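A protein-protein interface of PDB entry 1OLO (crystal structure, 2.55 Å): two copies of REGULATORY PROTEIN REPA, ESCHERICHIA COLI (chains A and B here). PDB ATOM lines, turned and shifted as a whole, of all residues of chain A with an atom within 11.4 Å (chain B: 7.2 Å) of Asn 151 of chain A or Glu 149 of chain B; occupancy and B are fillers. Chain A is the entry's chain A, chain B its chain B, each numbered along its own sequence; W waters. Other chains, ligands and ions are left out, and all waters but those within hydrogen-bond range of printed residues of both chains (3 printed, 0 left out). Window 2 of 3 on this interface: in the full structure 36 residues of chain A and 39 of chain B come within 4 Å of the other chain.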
ATOM      1  N   LEU A 142     -39.801  -7.910 -14.803  1.00  0.00           N
ATOM      2  CA  LEU A 142     -38.460  -7.756 -15.313  1.00  0.00           C
ATOM      3  C   LEU A 142     -37.749  -9.105 -15.363  1.00  0.00           C
ATOM      4  O   LEU A 142     -36.920  -9.294 -16.221  1.00  0.00           O
ATOM      5  CB  LEU A 142     -37.648  -6.805 -14.438  1.00  0.00           C
ATOM      6  CG  LEU A 142     -36.306  -6.390 -15.043  1.00  0.00           C
ATOM      7  CD1 LEU A 142     -36.529  -5.711 -16.453  1.00  0.00           C
ATOM      8  CD2 LEU A 142     -35.529  -5.520 -14.082  1.00  0.00           C
ATOM      9  N   ARG A 143     -38.048 -10.018 -14.447  1.00  0.00           N
ATOM     10  CA  ARG A 143     -37.291 -11.267 -14.345  1.00  0.00           C
ATOM     11  C   ARG A 143     -37.288 -12.040 -15.692  1.00  0.00           C
ATOM     12  O   ARG A 143     -36.384 -12.842 -16.002  1.00  0.00           O
ATOM     13  CB  ARG A 143     -37.839 -12.133 -13.223  1.00  0.00           C
ATOM     14  CG  ARG A 143     -37.138 -13.497 -13.046  1.00  0.00           C
ATOM     15  CD  ARG A 143     -35.671 -13.430 -12.624  1.00  0.00           C
ATOM     16  NE  ARG A 143     -34.808 -13.312 -13.799  1.00  0.00           N
ATOM     17  CZ  ARG A 143     -33.481 -13.387 -13.764  1.00  0.00           C
ATOM     18  NH1 ARG A 143     -32.831 -13.518 -12.593  1.00  0.00           N
ATOM     19  NH2 ARG A 143     -32.782 -13.265 -14.889  1.00  0.00           N
ATOM     20  N   HIS A 146     -34.579 -10.743 -19.025  1.00  0.00           N
ATOM     21  CA  HIS A 146     -33.125 -10.796 -18.946  1.00  0.00           C
ATOM     22  C   HIS A 146     -32.710 -12.102 -18.285  1.00  0.00           C
ATOM     23  O   HIS A 146     -33.508 -12.718 -17.582  1.00  0.00           O
ATOM     24  CB  HIS A 146     -32.545  -9.593 -18.198  1.00  0.00           C
ATOM     25  CG  HIS A 146     -32.686  -9.686 -16.710  1.00  0.00           C
ATOM     26  ND1 HIS A 146     -31.736 -10.294 -15.904  1.00  0.00           N
ATOM     27  CD2 HIS A 146     -33.700  -9.313 -15.889  1.00  0.00           C
ATOM     28  CE1 HIS A 146     -32.160 -10.281 -14.649  1.00  0.00           C
ATOM     29  NE2 HIS A 146     -33.334  -9.663 -14.607  1.00  0.00           N
ATOM     30  N   ILE A 147     -31.478 -12.529 -18.529  1.00  0.00           N
ATOM     31  CA  ILE A 147     -30.989 -13.767 -17.930  1.00  0.00           C
ATOM     32  C   ILE A 147     -29.797 -13.552 -17.000  1.00  0.00           C
ATOM     33  O   ILE A 147     -28.972 -14.462 -16.814  1.00  0.00           O
ATOM     34  CB  ILE A 147     -30.639 -14.791 -18.999  1.00  0.00           C
ATOM     35  CG1 ILE A 147     -29.552 -14.252 -19.956  1.00  0.00           C
ATOM     36  CG2 ILE A 147     -31.910 -15.239 -19.703  1.00  0.00           C
ATOM     37  CD1 ILE A 147     -28.939 -15.295 -20.917  1.00  0.00           C
ATOM     38  N   GLU A 148     -29.714 -12.350 -16.416  1.00  0.00           N
ATOM     39  CA  GLU A 148     -28.638 -12.034 -15.471  1.00  0.00           C
ATOM     40  C   GLU A 148     -29.065 -12.299 -14.052  1.00  0.00           C
ATOM     41  O   GLU A 148     -30.219 -12.615 -13.781  1.00  0.00           O
ATOM     42  CB  GLU A 148     -28.159 -10.597 -15.595  1.00  0.00           C
ATOM     43  CG  GLU A 148     -28.080 -10.050 -17.026  1.00  0.00           C
ATOM     44  CD  GLU A 148     -26.989 -10.701 -17.880  1.00  0.00           C
ATOM     45  OE1 GLU A 148     -25.991 -11.270 -17.312  1.00  0.00           O
ATOM     46  OE2 GLU A 148     -27.190 -10.660 -19.141  1.00  0.00           O
ATOM     47  N   GLU A 149     -28.095 -12.188 -13.171  1.00  0.00           N
ATOM     48  CA  GLU A 149     -28.260 -12.287 -11.747  1.00  0.00           C
ATOM     49  C   GLU A 149     -28.827 -10.951 -11.228  1.00  0.00           C
ATOM     50  O   GLU A 149     -28.170  -9.918 -11.405  1.00  0.00           O
ATOM     51  CB  GLU A 149     -26.848 -12.513 -11.202  1.00  0.00           C
ATOM     52  CG  GLU A 149     -26.757 -13.474 -10.044  1.00  0.00           C
ATOM     53  CD  GLU A 149     -27.390 -14.808 -10.346  1.00  0.00           C
ATOM     54  OE1 GLU A 149     -27.165 -15.394 -11.447  1.00  0.00           O
ATOM     55  OE2 GLU A 149     -28.147 -15.267  -9.477  1.00  0.00           O
ATOM     56  N   GLU A 150     -30.010 -10.967 -10.602  1.00  0.00           N
ATOM     57  CA  GLU A 150     -30.708  -9.766 -10.118  1.00  0.00           C
ATOM     58  C   GLU A 150     -30.054  -9.026  -8.945  1.00  0.00           C
ATOM     59  O   GLU A 150     -30.447  -7.894  -8.593  1.00  0.00           O
ATOM     60  CB  GLU A 150     -32.216 -10.019  -9.884  1.00  0.00           C
ATOM     61  CG  GLU A 150     -32.986  -9.854 -11.209  1.00  0.00           C
ATOM     62  CD  GLU A 150     -34.519  -9.910 -11.150  1.00  0.00           C
ATOM     63  OE1 GLU A 150     -35.122 -10.211 -10.078  1.00  0.00           O
ATOM     64  OE2 GLU A 150     -35.135  -9.665 -12.226  1.00  0.00           O
ATOM     65  N   ASN A 151     -29.044  -9.641  -8.341  1.00  0.00           N
ATOM     66  CA  ASN A 151     -28.352  -8.974  -7.270  1.00  0.00           C
ATOM     67  C   ASN A 151     -26.892  -8.773  -7.645  1.00  0.00           C
ATOM     68  O   ASN A 151     -26.044  -8.574  -6.773  1.00  0.00           O
ATOM     69  CB  ASN A 151     -28.552  -9.727  -5.939  1.00  0.00           C
ATOM     70  CG  ASN A 151     -27.830 -11.061  -5.898  1.00  0.00           C
ATOM     71  OD1 ASN A 151     -27.033 -11.395  -6.791  1.00  0.00           O
ATOM     72  ND2 ASN A 151     -28.104 -11.846  -4.847  1.00  0.00           N
ATOM     73  N   ALA A 152     -26.619  -8.886  -8.947  1.00  0.00           N
ATOM     74  CA  ALA A 152     -25.345  -8.494  -9.548  1.00  0.00           C
ATOM     75  C   ALA A 152     -25.513  -7.064 -10.133  1.00  0.00           C
ATOM     76  O   ALA A 152     -26.183  -6.867 -11.141  1.00  0.00           O
ATOM     77  CB  ALA A 152     -24.899  -9.504 -10.608  1.00  0.00           C
ATOM     78  N   SER A 153     -24.904  -6.073  -9.468  1.00  0.00           N
ATOM     79  CA  SER A 153     -25.137  -4.669  -9.776  1.00  0.00           C
ATOM     80  C   SER A 153     -24.670  -4.295 -11.168  1.00  0.00           C
ATOM     81  O   SER A 153     -25.337  -3.522 -11.854  1.00  0.00           O
ATOM     82  CB  SER A 153     -24.518  -3.754  -8.726  1.00  0.00           C
ATOM     83  OG  SER A 153     -23.101  -3.793  -8.764  1.00  0.00           O
ATOM     84  N   GLY A 154     -23.543  -4.868 -11.582  1.00  0.00           N
ATOM     85  CA  GLY A 154     -22.999  -4.619 -12.910  1.00  0.00           C
ATOM     86  C   GLY A 154     -23.994  -4.987 -13.995  1.00  0.00           C
ATOM     87  O   GLY A 154     -24.444  -4.107 -14.728  1.00  0.00           O
ATOM     88  N   PRO A 155     -24.340  -6.278 -14.107  1.00  0.00           N
ATOM     89  CA  PRO A 155     -25.309  -6.724 -15.130  1.00  0.00           C
ATOM     90  C   PRO A 155     -26.629  -6.025 -15.014  1.00  0.00           C
ATOM     91  O   PRO A 155     -27.180  -5.682 -16.076  1.00  0.00           O
ATOM     92  CB  PRO A 155     -25.428  -8.246 -14.897  1.00  0.00           C
ATOM     93  CG  PRO A 155     -24.000  -8.612 -14.274  1.00  0.00           C
ATOM     94  CD  PRO A 155     -23.790  -7.420 -13.343  1.00  0.00           C
ATOM     95  N   MET A 156     -27.116  -5.774 -13.800  1.00  0.00           N
ATOM     96  CA  MET A 156     -28.361  -5.025 -13.673  1.00  0.00           C
ATOM     97  C   MET A 156     -28.277  -3.542 -14.155  1.00  0.00           C
ATOM     98  O   MET A 156     -29.276  -2.973 -14.632  1.00  0.00           O
ATOM     99  CB  MET A 156     -28.953  -5.139 -12.261  1.00  0.00           C
ATOM    100  CG  MET A 156     -29.463  -6.560 -11.899  1.00  0.00           C
ATOM    101  SD  MET A 156     -30.280  -7.524 -13.220  1.00  0.00           S
ATOM    102  CE  MET A 156     -31.660  -6.679 -13.331  1.00  0.00           C
ATOM    103  N   ALA A 157     -27.098  -2.930 -14.025  1.00  0.00           N
ATOM    104  CA  ALA A 157     -26.895  -1.584 -14.531  1.00  0.00           C
ATOM    105  C   ALA A 157     -27.047  -1.639 -16.080  1.00  0.00           C
ATOM    106  O   ALA A 157     -27.649  -0.744 -16.674  1.00  0.00           O
ATOM    107  CB  ALA A 157     -25.525  -1.018 -14.082  1.00  0.00           C
ATOM    108  N   GLN A 158     -26.555  -2.713 -16.704  1.00  0.00           N
ATOM    109  CA  GLN A 158     -26.683  -2.864 -18.116  1.00  0.00           C
ATOM    110  C   GLN A 158     -28.129  -3.011 -18.542  1.00  0.00           C
ATOM    111  O   GLN A 158     -28.586  -2.319 -19.477  1.00  0.00           O
ATOM    112  CB  GLN A 158     -25.871  -4.020 -18.587  1.00  0.00           C
ATOM    113  CG  GLN A 158     -24.372  -3.784 -18.453  1.00  0.00           C
ATOM    114  CD  GLN A 158     -23.572  -5.013 -18.902  1.00  0.00           C
ATOM    115  OE1 GLN A 158     -23.210  -5.138 -20.077  1.00  0.00           O
ATOM    116  NE2 GLN A 158     -23.324  -5.926 -17.979  1.00  0.00           N
ATOM    117  N   VAL A 159     -28.859  -3.876 -17.837  1.00  0.00           N
ATOM    118  CA  VAL A 159     -30.287  -4.105 -18.128  1.00  0.00           C
ATOM    119  C   VAL A 159     -31.063  -2.826 -17.974  1.00  0.00           C
ATOM    120  O   VAL A 159     -31.813  -2.441 -18.863  1.00  0.00           O
ATOM    121  CB  VAL A 159     -30.881  -5.235 -17.277  1.00  0.00           C
ATOM    122  CG1 VAL A 159     -32.445  -5.269 -17.390  1.00  0.00           C
ATOM    123  CG2 VAL A 159     -30.234  -6.591 -17.684  1.00  0.00           C
ATOM    124  N   ILE A 160     -30.843  -2.131 -16.869  1.00  0.00           N
ATOM    125  CA  ILE A 160     -31.515  -0.884 -16.652  1.00  0.00           C
ATOM    126  C   ILE A 160     -31.067   0.228 -17.607  1.00  0.00           C
ATOM    127  O   ILE A 160     -31.895   1.036 -18.053  1.00  0.00           O
ATOM    128  CB  ILE A 160     -31.353  -0.468 -15.173  1.00  0.00           C
ATOM    129  CG1 ILE A 160     -32.495  -1.080 -14.392  1.00  0.00           C
ATOM    130  CG2 ILE A 160     -31.313   1.091 -14.987  1.00  0.00           C
ATOM    131  CD1 ILE A 160     -32.008  -1.695 -13.161  1.00  0.00           C
ATOM    132  N   HIS A 178     -41.568  -5.959 -10.399  1.00  0.00           N
ATOM    133  CA  HIS A 178     -40.561  -6.782  -9.825  1.00  0.00           C
ATOM    134  C   HIS A 178     -41.126  -7.520  -8.613  1.00  0.00           C
ATOM    135  O   HIS A 178     -41.723  -6.873  -7.731  1.00  0.00           O
ATOM    136  CB  HIS A 178     -39.439  -5.852  -9.395  1.00  0.00           C
ATOM    137  CG  HIS A 178     -38.341  -6.538  -8.673  1.00  0.00           C
ATOM    138  ND1 HIS A 178     -37.554  -7.507  -9.264  1.00  0.00           N
ATOM    139  CD2 HIS A 178     -37.877  -6.395  -7.406  1.00  0.00           C
ATOM    140  CE1 HIS A 178     -36.642  -7.915  -8.398  1.00  0.00           C
ATOM    141  NE2 HIS A 178     -36.825  -7.269  -7.258  1.00  0.00           N
ATOM    142  N   HIS A 179     -40.947  -8.854  -8.562  1.00  0.00           N
ATOM    143  CA  HIS A 179     -41.341  -9.671  -7.392  1.00  0.00           C
ATOM    144  C   HIS A 179     -40.278  -9.520  -6.287  1.00  0.00           C
ATOM    145  O   HIS A 179     -39.103  -9.802  -6.526  1.00  0.00           O
ATOM    146  CB  HIS A 179     -41.513 -11.144  -7.772  1.00  0.00           C
ATOM    147  CG  HIS A 179     -42.534 -11.410  -8.845  1.00  0.00           C
ATOM    148  ND1 HIS A 179     -43.840 -10.950  -8.791  1.00  0.00           N
ATOM    149  CD2 HIS A 179     -42.451 -12.151  -9.987  1.00  0.00           C
ATOM    150  CE1 HIS A 179     -44.505 -11.385  -9.850  1.00  0.00           C
ATOM    151  NE2 HIS A 179     -43.687 -12.119 -10.590  1.00  0.00           N
ATOM    152  N   ALA A 180     -40.668  -9.059  -5.098  1.00  0.00           N
ATOM    153  CA  ALA A 180     -39.716  -8.786  -3.977  1.00  0.00           C
ATOM    154  C   ALA A 180     -39.298 -10.120  -3.420  1.00  0.00           C
ATOM    155  O   ALA A 180     -40.177 -10.843  -2.887  1.00  0.00           O
ATOM    156  CB  ALA A 180     -40.412  -7.998  -2.849  1.00  0.00           C
ATOM    157  N   VAL A 201     -31.148  -3.463  -4.982  1.00  0.00           N
ATOM    158  CA  VAL A 201     -30.034  -3.273  -5.934  1.00  0.00           C
ATOM    159  C   VAL A 201     -30.662  -2.850  -7.246  1.00  0.00           C
ATOM    160  O   VAL A 201     -30.265  -1.892  -7.933  1.00  0.00           O
ATOM    161  CB  VAL A 201     -29.258  -4.634  -6.234  1.00  0.00           C
ATOM    162  CG1 VAL A 201     -28.759  -4.740  -7.766  1.00  0.00           C
ATOM    163  CG2 VAL A 201     -28.107  -4.911  -5.205  1.00  0.00           C
ATOM    164  N   LEU A 202     -31.669  -3.617  -7.602  1.00  0.00           N
ATOM    165  CA  LEU A 202     -32.557  -3.233  -8.689  1.00  0.00           C
ATOM    166  C   LEU A 202     -33.333  -1.973  -8.332  1.00  0.00           C
ATOM    167  O   LEU A 202     -33.822  -1.286  -9.218  1.00  0.00           O
ATOM    168  CB  LEU A 202     -33.536  -4.366  -8.943  1.00  0.00           C
ATOM    169  CG  LEU A 202     -34.050  -4.563 -10.340  1.00  0.00           C
ATOM    170  CD1 LEU A 202     -33.135  -3.986 -11.453  1.00  0.00           C
ATOM    171  CD2 LEU A 202     -34.424  -6.054 -10.543  1.00  0.00           C
ATOM    172  N   VAL A 203     -33.450  -1.660  -7.051  1.00  0.00           N
ATOM    173  CA  VAL A 203     -34.276  -0.541  -6.670  1.00  0.00           C
ATOM    174  C   VAL A 203     -33.422   0.667  -6.299  1.00  0.00           C
ATOM    175  O   VAL A 203     -33.839   1.803  -6.556  1.00  0.00           O
ATOM    176  CB  VAL A 203     -35.349  -0.930  -5.551  1.00  0.00           C
ATOM    177  CG1 VAL A 203     -35.997  -2.345  -5.823  1.00  0.00           C
ATOM    178  CG2 VAL A 203     -34.818  -0.753  -4.043  1.00  0.00           C
ATOM    179  N   ASP A 204     -32.229   0.438  -5.739  1.00  0.00           N
ATOM    180  CA  ASP A 204     -31.317   1.542  -5.403  1.00  0.00           C
ATOM    181  C   ASP A 204     -31.007   2.590  -6.481  1.00  0.00           C
ATOM    182  O   ASP A 204     -30.737   3.750  -6.141  1.00  0.00           O
ATOM    183  CB  ASP A 204     -30.017   1.025  -4.781  1.00  0.00           C
ATOM    184  CG  ASP A 204     -30.287   0.122  -3.577  1.00  0.00           C
ATOM    185  OD1 ASP A 204     -29.408  -0.693  -3.183  1.00  0.00           O
ATOM    186  OD2 ASP A 204     -31.399   0.149  -2.984  1.00  0.00           O
ATOM    187  N   ASN A 205     -31.056   2.193  -7.745  1.00  0.00           N
ATOM    188  CA  ASN A 205     -30.707   3.057  -8.846  1.00  0.00           C
ATOM    189  C   ASN A 205     -31.871   3.240  -9.852  1.00  0.00           C
ATOM    190  O   ASN A 205     -31.662   3.517 -11.040  1.00  0.00           O
ATOM    191  CB  ASN A 205     -29.447   2.503  -9.515  1.00  0.00           C
ATOM    192  CG  ASN A 205     -28.191   2.620  -8.606  1.00  0.00           C
ATOM    193  OD1 ASN A 205     -27.571   3.710  -8.468  1.00  0.00           O
ATOM    194  ND2 ASN A 205     -27.835   1.508  -7.948  1.00  0.00           N
ATOM    195  N   ARG B 143     -23.063   5.132 -10.654  1.00  0.00           N
ATOM    196  CA  ARG B 143     -23.633   3.908 -11.179  1.00  0.00           C
ATOM    197  C   ARG B 143     -23.880   3.901 -12.722  1.00  0.00           C
ATOM    198  O   ARG B 143     -23.817   2.816 -13.365  1.00  0.00           O
ATOM    199  CB  ARG B 143     -24.917   3.561 -10.419  1.00  0.00           C
ATOM    200  CG  ARG B 143     -25.633   2.295 -10.869  1.00  0.00           C
ATOM    201  CD  ARG B 143     -24.911   1.006 -10.502  1.00  0.00           C
ATOM    202  NE  ARG B 143     -23.907   0.693 -11.521  1.00  0.00           N
ATOM    203  CZ  ARG B 143     -23.128  -0.355 -11.493  1.00  0.00           C
ATOM    204  NH1 ARG B 143     -23.187  -1.191 -10.464  1.00  0.00           N
ATOM    205  NH2 ARG B 143     -22.283  -0.566 -12.500  1.00  0.00           N
ATOM    206  N   HIS B 146     -20.499   3.192 -15.447  1.00  0.00           N
ATOM    207  CA  HIS B 146     -19.708   1.981 -15.493  1.00  0.00           C
ATOM    208  C   HIS B 146     -20.649   0.800 -15.291  1.00  0.00           C
ATOM    209  O   HIS B 146     -21.742   0.942 -14.733  1.00  0.00           O
ATOM    210  CB  HIS B 146     -18.597   1.987 -14.426  1.00  0.00           C
ATOM    211  CG  HIS B 146     -19.101   1.693 -13.043  1.00  0.00           C
ATOM    212  ND1 HIS B 146     -19.091   0.418 -12.497  1.00  0.00           N
ATOM    213  CD2 HIS B 146     -19.706   2.492 -12.123  1.00  0.00           C
ATOM    214  CE1 HIS B 146     -19.630   0.452 -11.288  1.00  0.00           C
ATOM    215  NE2 HIS B 146     -19.986   1.706 -11.025  1.00  0.00           N
ATOM    216  N   ILE B 147     -20.179  -0.367 -15.733  1.00  0.00           N
ATOM    217  CA  ILE B 147     -20.933  -1.608 -15.685  1.00  0.00           C
ATOM    218  C   ILE B 147     -20.250  -2.653 -14.798  1.00  0.00           C
ATOM    219  O   ILE B 147     -20.500  -3.894 -14.938  1.00  0.00           O
ATOM    220  CB  ILE B 147     -21.153  -2.153 -17.108  1.00  0.00           C
ATOM    221  CG1 ILE B 147     -19.819  -2.353 -17.819  1.00  0.00           C
ATOM    222  CG2 ILE B 147     -22.033  -1.188 -17.916  1.00  0.00           C
ATOM    223  CD1 ILE B 147     -19.851  -3.366 -18.938  1.00  0.00           C
ATOM    224  N   GLU B 148     -19.426  -2.164 -13.861  1.00  0.00           N
ATOM    225  CA  GLU B 148     -18.792  -3.084 -12.894  1.00  0.00           C
ATOM    226  C   GLU B 148     -19.645  -3.353 -11.654  1.00  0.00           C
ATOM    227  O   GLU B 148     -20.589  -2.625 -11.349  1.00  0.00           O
ATOM    228  CB  GLU B 148     -17.410  -2.576 -12.491  1.00  0.00           C
ATOM    229  CG  GLU B 148     -16.484  -2.214 -13.662  1.00  0.00           C
ATOM    230  CD  GLU B 148     -16.336  -3.302 -14.708  1.00  0.00           C
ATOM    231  OE1 GLU B 148     -16.312  -4.551 -14.384  1.00  0.00           O
ATOM    232  OE2 GLU B 148     -16.283  -2.862 -15.895  1.00  0.00           O
ATOM    233  N   GLU B 149     -19.288  -4.398 -10.945  1.00  0.00           N
ATOM    234  CA  GLU B 149     -19.834  -4.708  -9.644  1.00  0.00           C
ATOM    235  C   GLU B 149     -19.299  -3.711  -8.600  1.00  0.00           C
ATOM    236  O   GLU B 149     -18.098  -3.686  -8.320  1.00  0.00           O
ATOM    237  CB  GLU B 149     -19.407  -6.114  -9.328  1.00  0.00           C
ATOM    238  CG  GLU B 149     -20.363  -6.807  -8.418  1.00  0.00           C
ATOM    239  CD  GLU B 149     -21.740  -7.005  -9.050  1.00  0.00           C
ATOM    240  OE1 GLU B 149     -21.842  -7.160 -10.322  1.00  0.00           O
ATOM    241  OE2 GLU B 149     -22.730  -7.009  -8.251  1.00  0.00           O
ATOM    242  N   GLU B 150     -20.189  -2.875  -8.055  1.00  0.00           N
ATOM    243  CA  GLU B 150     -19.821  -1.806  -7.112  1.00  0.00           C
ATOM    244  C   GLU B 150     -19.266  -2.348  -5.782  1.00  0.00           C
ATOM    245  O   GLU B 150     -18.526  -1.664  -5.042  1.00  0.00           O
ATOM    246  CB  GLU B 150     -20.965  -0.808  -6.883  1.00  0.00           C
ATOM    247  CG  GLU B 150     -20.985   0.184  -8.010  1.00  0.00           C
ATOM    248  CD  GLU B 150     -21.911   1.407  -7.842  1.00  0.00           C
ATOM    249  OE1 GLU B 150     -22.765   1.346  -6.890  1.00  0.00           O
ATOM    250  OE2 GLU B 150     -21.774   2.393  -8.684  1.00  0.00           O
ATOM    251  N   ASN B 151     -19.594  -3.597  -5.504  1.00  0.00           N
ATOM    252  CA  ASN B 151     -19.070  -4.260  -4.339  1.00  0.00           C
ATOM    253  C   ASN B 151     -17.787  -5.093  -4.628  1.00  0.00           C
ATOM    254  O   ASN B 151     -17.327  -5.844  -3.756  1.00  0.00           O
ATOM    255  CB  ASN B 151     -20.215  -5.051  -3.663  1.00  0.00           C
ATOM    256  CG  ASN B 151     -20.389  -6.452  -4.253  1.00  0.00           C
ATOM    257  OD1 ASN B 151     -19.611  -6.879  -5.131  1.00  0.00           O
ATOM    258  ND2 ASN B 151     -21.398  -7.201  -3.757  1.00  0.00           N
ATOM    259  N   ALA B 152     -17.233  -4.992  -5.847  1.00  0.00           N
ATOM    260  CA  ALA B 152     -15.976  -5.673  -6.145  1.00  0.00           C
ATOM    261  C   ALA B 152     -14.848  -4.626  -6.162  1.00  0.00           C
ATOM    262  O   ALA B 152     -14.907  -3.616  -6.876  1.00  0.00           O
ATOM    263  CB  ALA B 152     -16.051  -6.486  -7.416  1.00  0.00           C
ATOM    264  N   SER B 153     -13.834  -4.841  -5.330  1.00  0.00           N
ATOM    265  CA  SER B 153     -12.874  -3.791  -5.029  1.00  0.00           C
ATOM    266  C   SER B 153     -11.854  -3.594  -6.163  1.00  0.00           C
ATOM    267  O   SER B 153     -11.404  -2.455  -6.397  1.00  0.00           O
ATOM    268  CB  SER B 153     -12.180  -4.064  -3.694  1.00  0.00           C
ATOM    269  OG  SER B 153     -11.470  -5.310  -3.765  1.00  0.00           O
ATOM    270  N   GLY B 154     -11.512  -4.700  -6.836  1.00  0.00           N
ATOM    271  CA  GLY B 154     -10.679  -4.692  -8.025  1.00  0.00           C
ATOM    272  C   GLY B 154     -11.235  -3.825  -9.156  1.00  0.00           C
ATOM    273  O   GLY B 154     -10.625  -2.808  -9.531  1.00  0.00           O
ATOM    274  N   PRO B 155     -12.382  -4.230  -9.714  1.00  0.00           N
ATOM    275  CA  PRO B 155     -13.069  -3.411 -10.738  1.00  0.00           C
ATOM    276  C   PRO B 155     -13.341  -2.037 -10.258  1.00  0.00           C
ATOM    277  O   PRO B 155     -13.134  -1.087 -11.044  1.00  0.00           O
ATOM    278  CB  PRO B 155     -14.365  -4.181 -11.031  1.00  0.00           C
ATOM    279  CG  PRO B 155     -14.005  -5.633 -10.649  1.00  0.00           C
ATOM    280  CD  PRO B 155     -13.040  -5.544  -9.494  1.00  0.00           C
ATOM    281  N   MET B 156     -13.746  -1.867  -8.998  1.00  0.00           N
ATOM    282  CA  MET B 156     -13.913  -0.476  -8.563  1.00  0.00           C
ATOM    283  C   MET B 156     -12.588   0.312  -8.441  1.00  0.00           C
ATOM    284  O   MET B 156     -12.586   1.523  -8.575  1.00  0.00           O
ATOM    285  CB  MET B 156     -14.769  -0.372  -7.323  1.00  0.00           C
ATOM    286  CG  MET B 156     -16.204  -0.801  -7.511  1.00  0.00           C
ATOM    287  SD  MET B 156     -17.052  -0.134  -9.001  1.00  0.00           S
ATOM    288  CE  MET B 156     -17.055   1.568  -8.690  1.00  0.00           C
ATOM    289  N   LEU B 202     -16.530   1.435  -2.316  1.00  0.00           N
ATOM    290  CA  LEU B 202     -16.230   2.736  -2.866  1.00  0.00           C
ATOM    291  C   LEU B 202     -15.676   3.565  -1.747  1.00  0.00           C
ATOM    292  O   LEU B 202     -14.589   4.087  -1.867  1.00  0.00           O
ATOM    293  CB  LEU B 202     -17.475   3.398  -3.432  1.00  0.00           C
ATOM    294  CG  LEU B 202     -17.745   3.016  -4.885  1.00  0.00           C
ATOM    295  CD1 LEU B 202     -17.926   1.509  -4.982  1.00  0.00           C
ATOM    296  CD2 LEU B 202     -19.002   3.720  -5.381  1.00  0.00           C
HETATM  297  O   HOH W   1     -25.089   2.459  -6.712  1.00  0.00           O
HETATM  298  O   HOH W   2     -21.570  -6.067 -16.117  1.00  0.00           O
HETATM  299  O   HOH W   3     -22.190  -5.052  -6.351  1.00  0.00           O
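OG of Ser 153 of chain A is in hydrogen-bond range of NH1 of Arg 143 of chain B (3.1 Å). OG of Ser 153 of chain A sits at hydrogen-bond distance from N of Glu 150 of chain B, at 3.1 Å. N of Ser 153 of chain A sits at hydrogen-bond distance from OE2 of Glu 149 of chain B (2.7 Å). OE1 of Glu 149 of chain B lies within hydrogen-bond range of N of Gly 154 of chain A (3.1 Å).
The backbone carbonyl oxygen (O) of Glu 148 of chain B is in hydrogen-bond range of the guanidinium group (NH2) of Arg 143 of chain B (2.9 Å). A ring nitrogen (ND1) of His 146 of chain B sits at hydrogen-bond distance from the backbone NH (N) of Glu 148 of chain B (2.9 Å). The backbone carbonyl oxygen (O) of His 146 of chain B sits at hydrogen-bond distance from the guanidinium group (NH2) of Arg 143 of chain B (2.7 Å). The guanidinium group (NE) of Arg 143 of chain B is in salt-bridge range of the side-chain carboxylate (OE2) of Glu 150 of chain B (3.9 Å).
Among the printed residues, merely in contact across the chains: Asn 151 of chain A with Glu 149 of chain B (3.95 Å), Ala 152 of chain A with Glu 149 of chain B (3.3 Å), Ser 153 of chain A with Glu 148 of chain B (3.8 Å), Gly 154 of chain A with Arg 143 of chain B (3.9 Å), Gly 154 of chain A with Ile 147 of chain B (3.3 Å), Gly 154 of chain A with Glu 148 of chain B (3.5 Å), Pro 155 of chain A with Glu 149 of chain B (3.6 Å), Ala 157 of chain A with Arg 143 of chain B (3.5 Å), Gln 158 of chain A with Ile 147 of chain B (3.5 Å) and Asn 205 of chain A with Arg 143 of chain B (3.3 Å).
Asn 151 of chain A touches just one residue of chain B: Glu 149. Printed residues of chain B within 4 Å of Ala 152 of chain A: Glu 149 (3.3 Å). Printed residues of chain B within 4 Å of Gly 154 of chain A: Arg 143, Ile 147, Glu 148 and Glu 149. Of chain A, only Ser 153 (3.8 Å) and Gly 154 (3.5 Å) come within 4 Å of Glu 148 of chain B. Glu 150 of chain B touches just one residue of chain A: Ser 153. Asn 151 of chain B touches none of the printed residues of chain A. No residue of chain A comes within 4 Å of Ala 152 of chain B. No residue of chain A comes within 4 Å of Pro 155 of chain B. The nearest printed residue of chain A that does not touch Glu 149 of chain B is Val 201 of chain A (6.5 Å). The nearest printed residue of chain A that does not touch Arg 143 of chain B is Pro 155 of chain A (6.3 Å).
Hydrophobic or aromatic side chains of chain B that line the printed part of chain A: Ile 147. Of the 25 printed residues of chain A, 8 touch a printed residue of chain B. Among the printed residues, 14 pairs touch across the chains. Among the printed residues, no Asp or Glu carboxylate lies within 4 Å of a Lys or Arg side-chain nitrogen of the other chain.
Ser 153 of chain A touches Glu 149 of chain B, but with the chains exchanged Glu 149 of chain A does not touch Ser 153 of chain B (16.2 Å). Gly 154 of chain A touches Ile 147 of chain B, but with the chains exchanged Ile 147 of chain A does not touch Gly 154 of chain B (22.1 Å). Gly 154 of chain A touches Glu 148 of chain B, but with the chains exchanged Glu 148 of chain A does not touch Gly 154 of chain B (18.4 Å). 13 positions are printed for both chains.
Water W2 lies within hydrogen-bond range of NE2 of Gln 158 of chain A (2.6 Å) and O of Ile 147 of chain B (2.7 Å). Water W1 lies within hydrogen-bond range of the side-chain carboxylate (OE1) of Glu 150 of chain B (2.6 Å) and the side-chain amide nitrogen (ND2) of Asn 205 of chain A (3.2 Å). Water W3 lies within hydrogen-bond range of OE2 of Glu 149 of chain B (2.8 Å), OG of Ser 153 of chain A (2.9 Å), N of Asn 151 of chain B (3.1 Å) and N of Glu 150 of chain B (3.4 Å).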
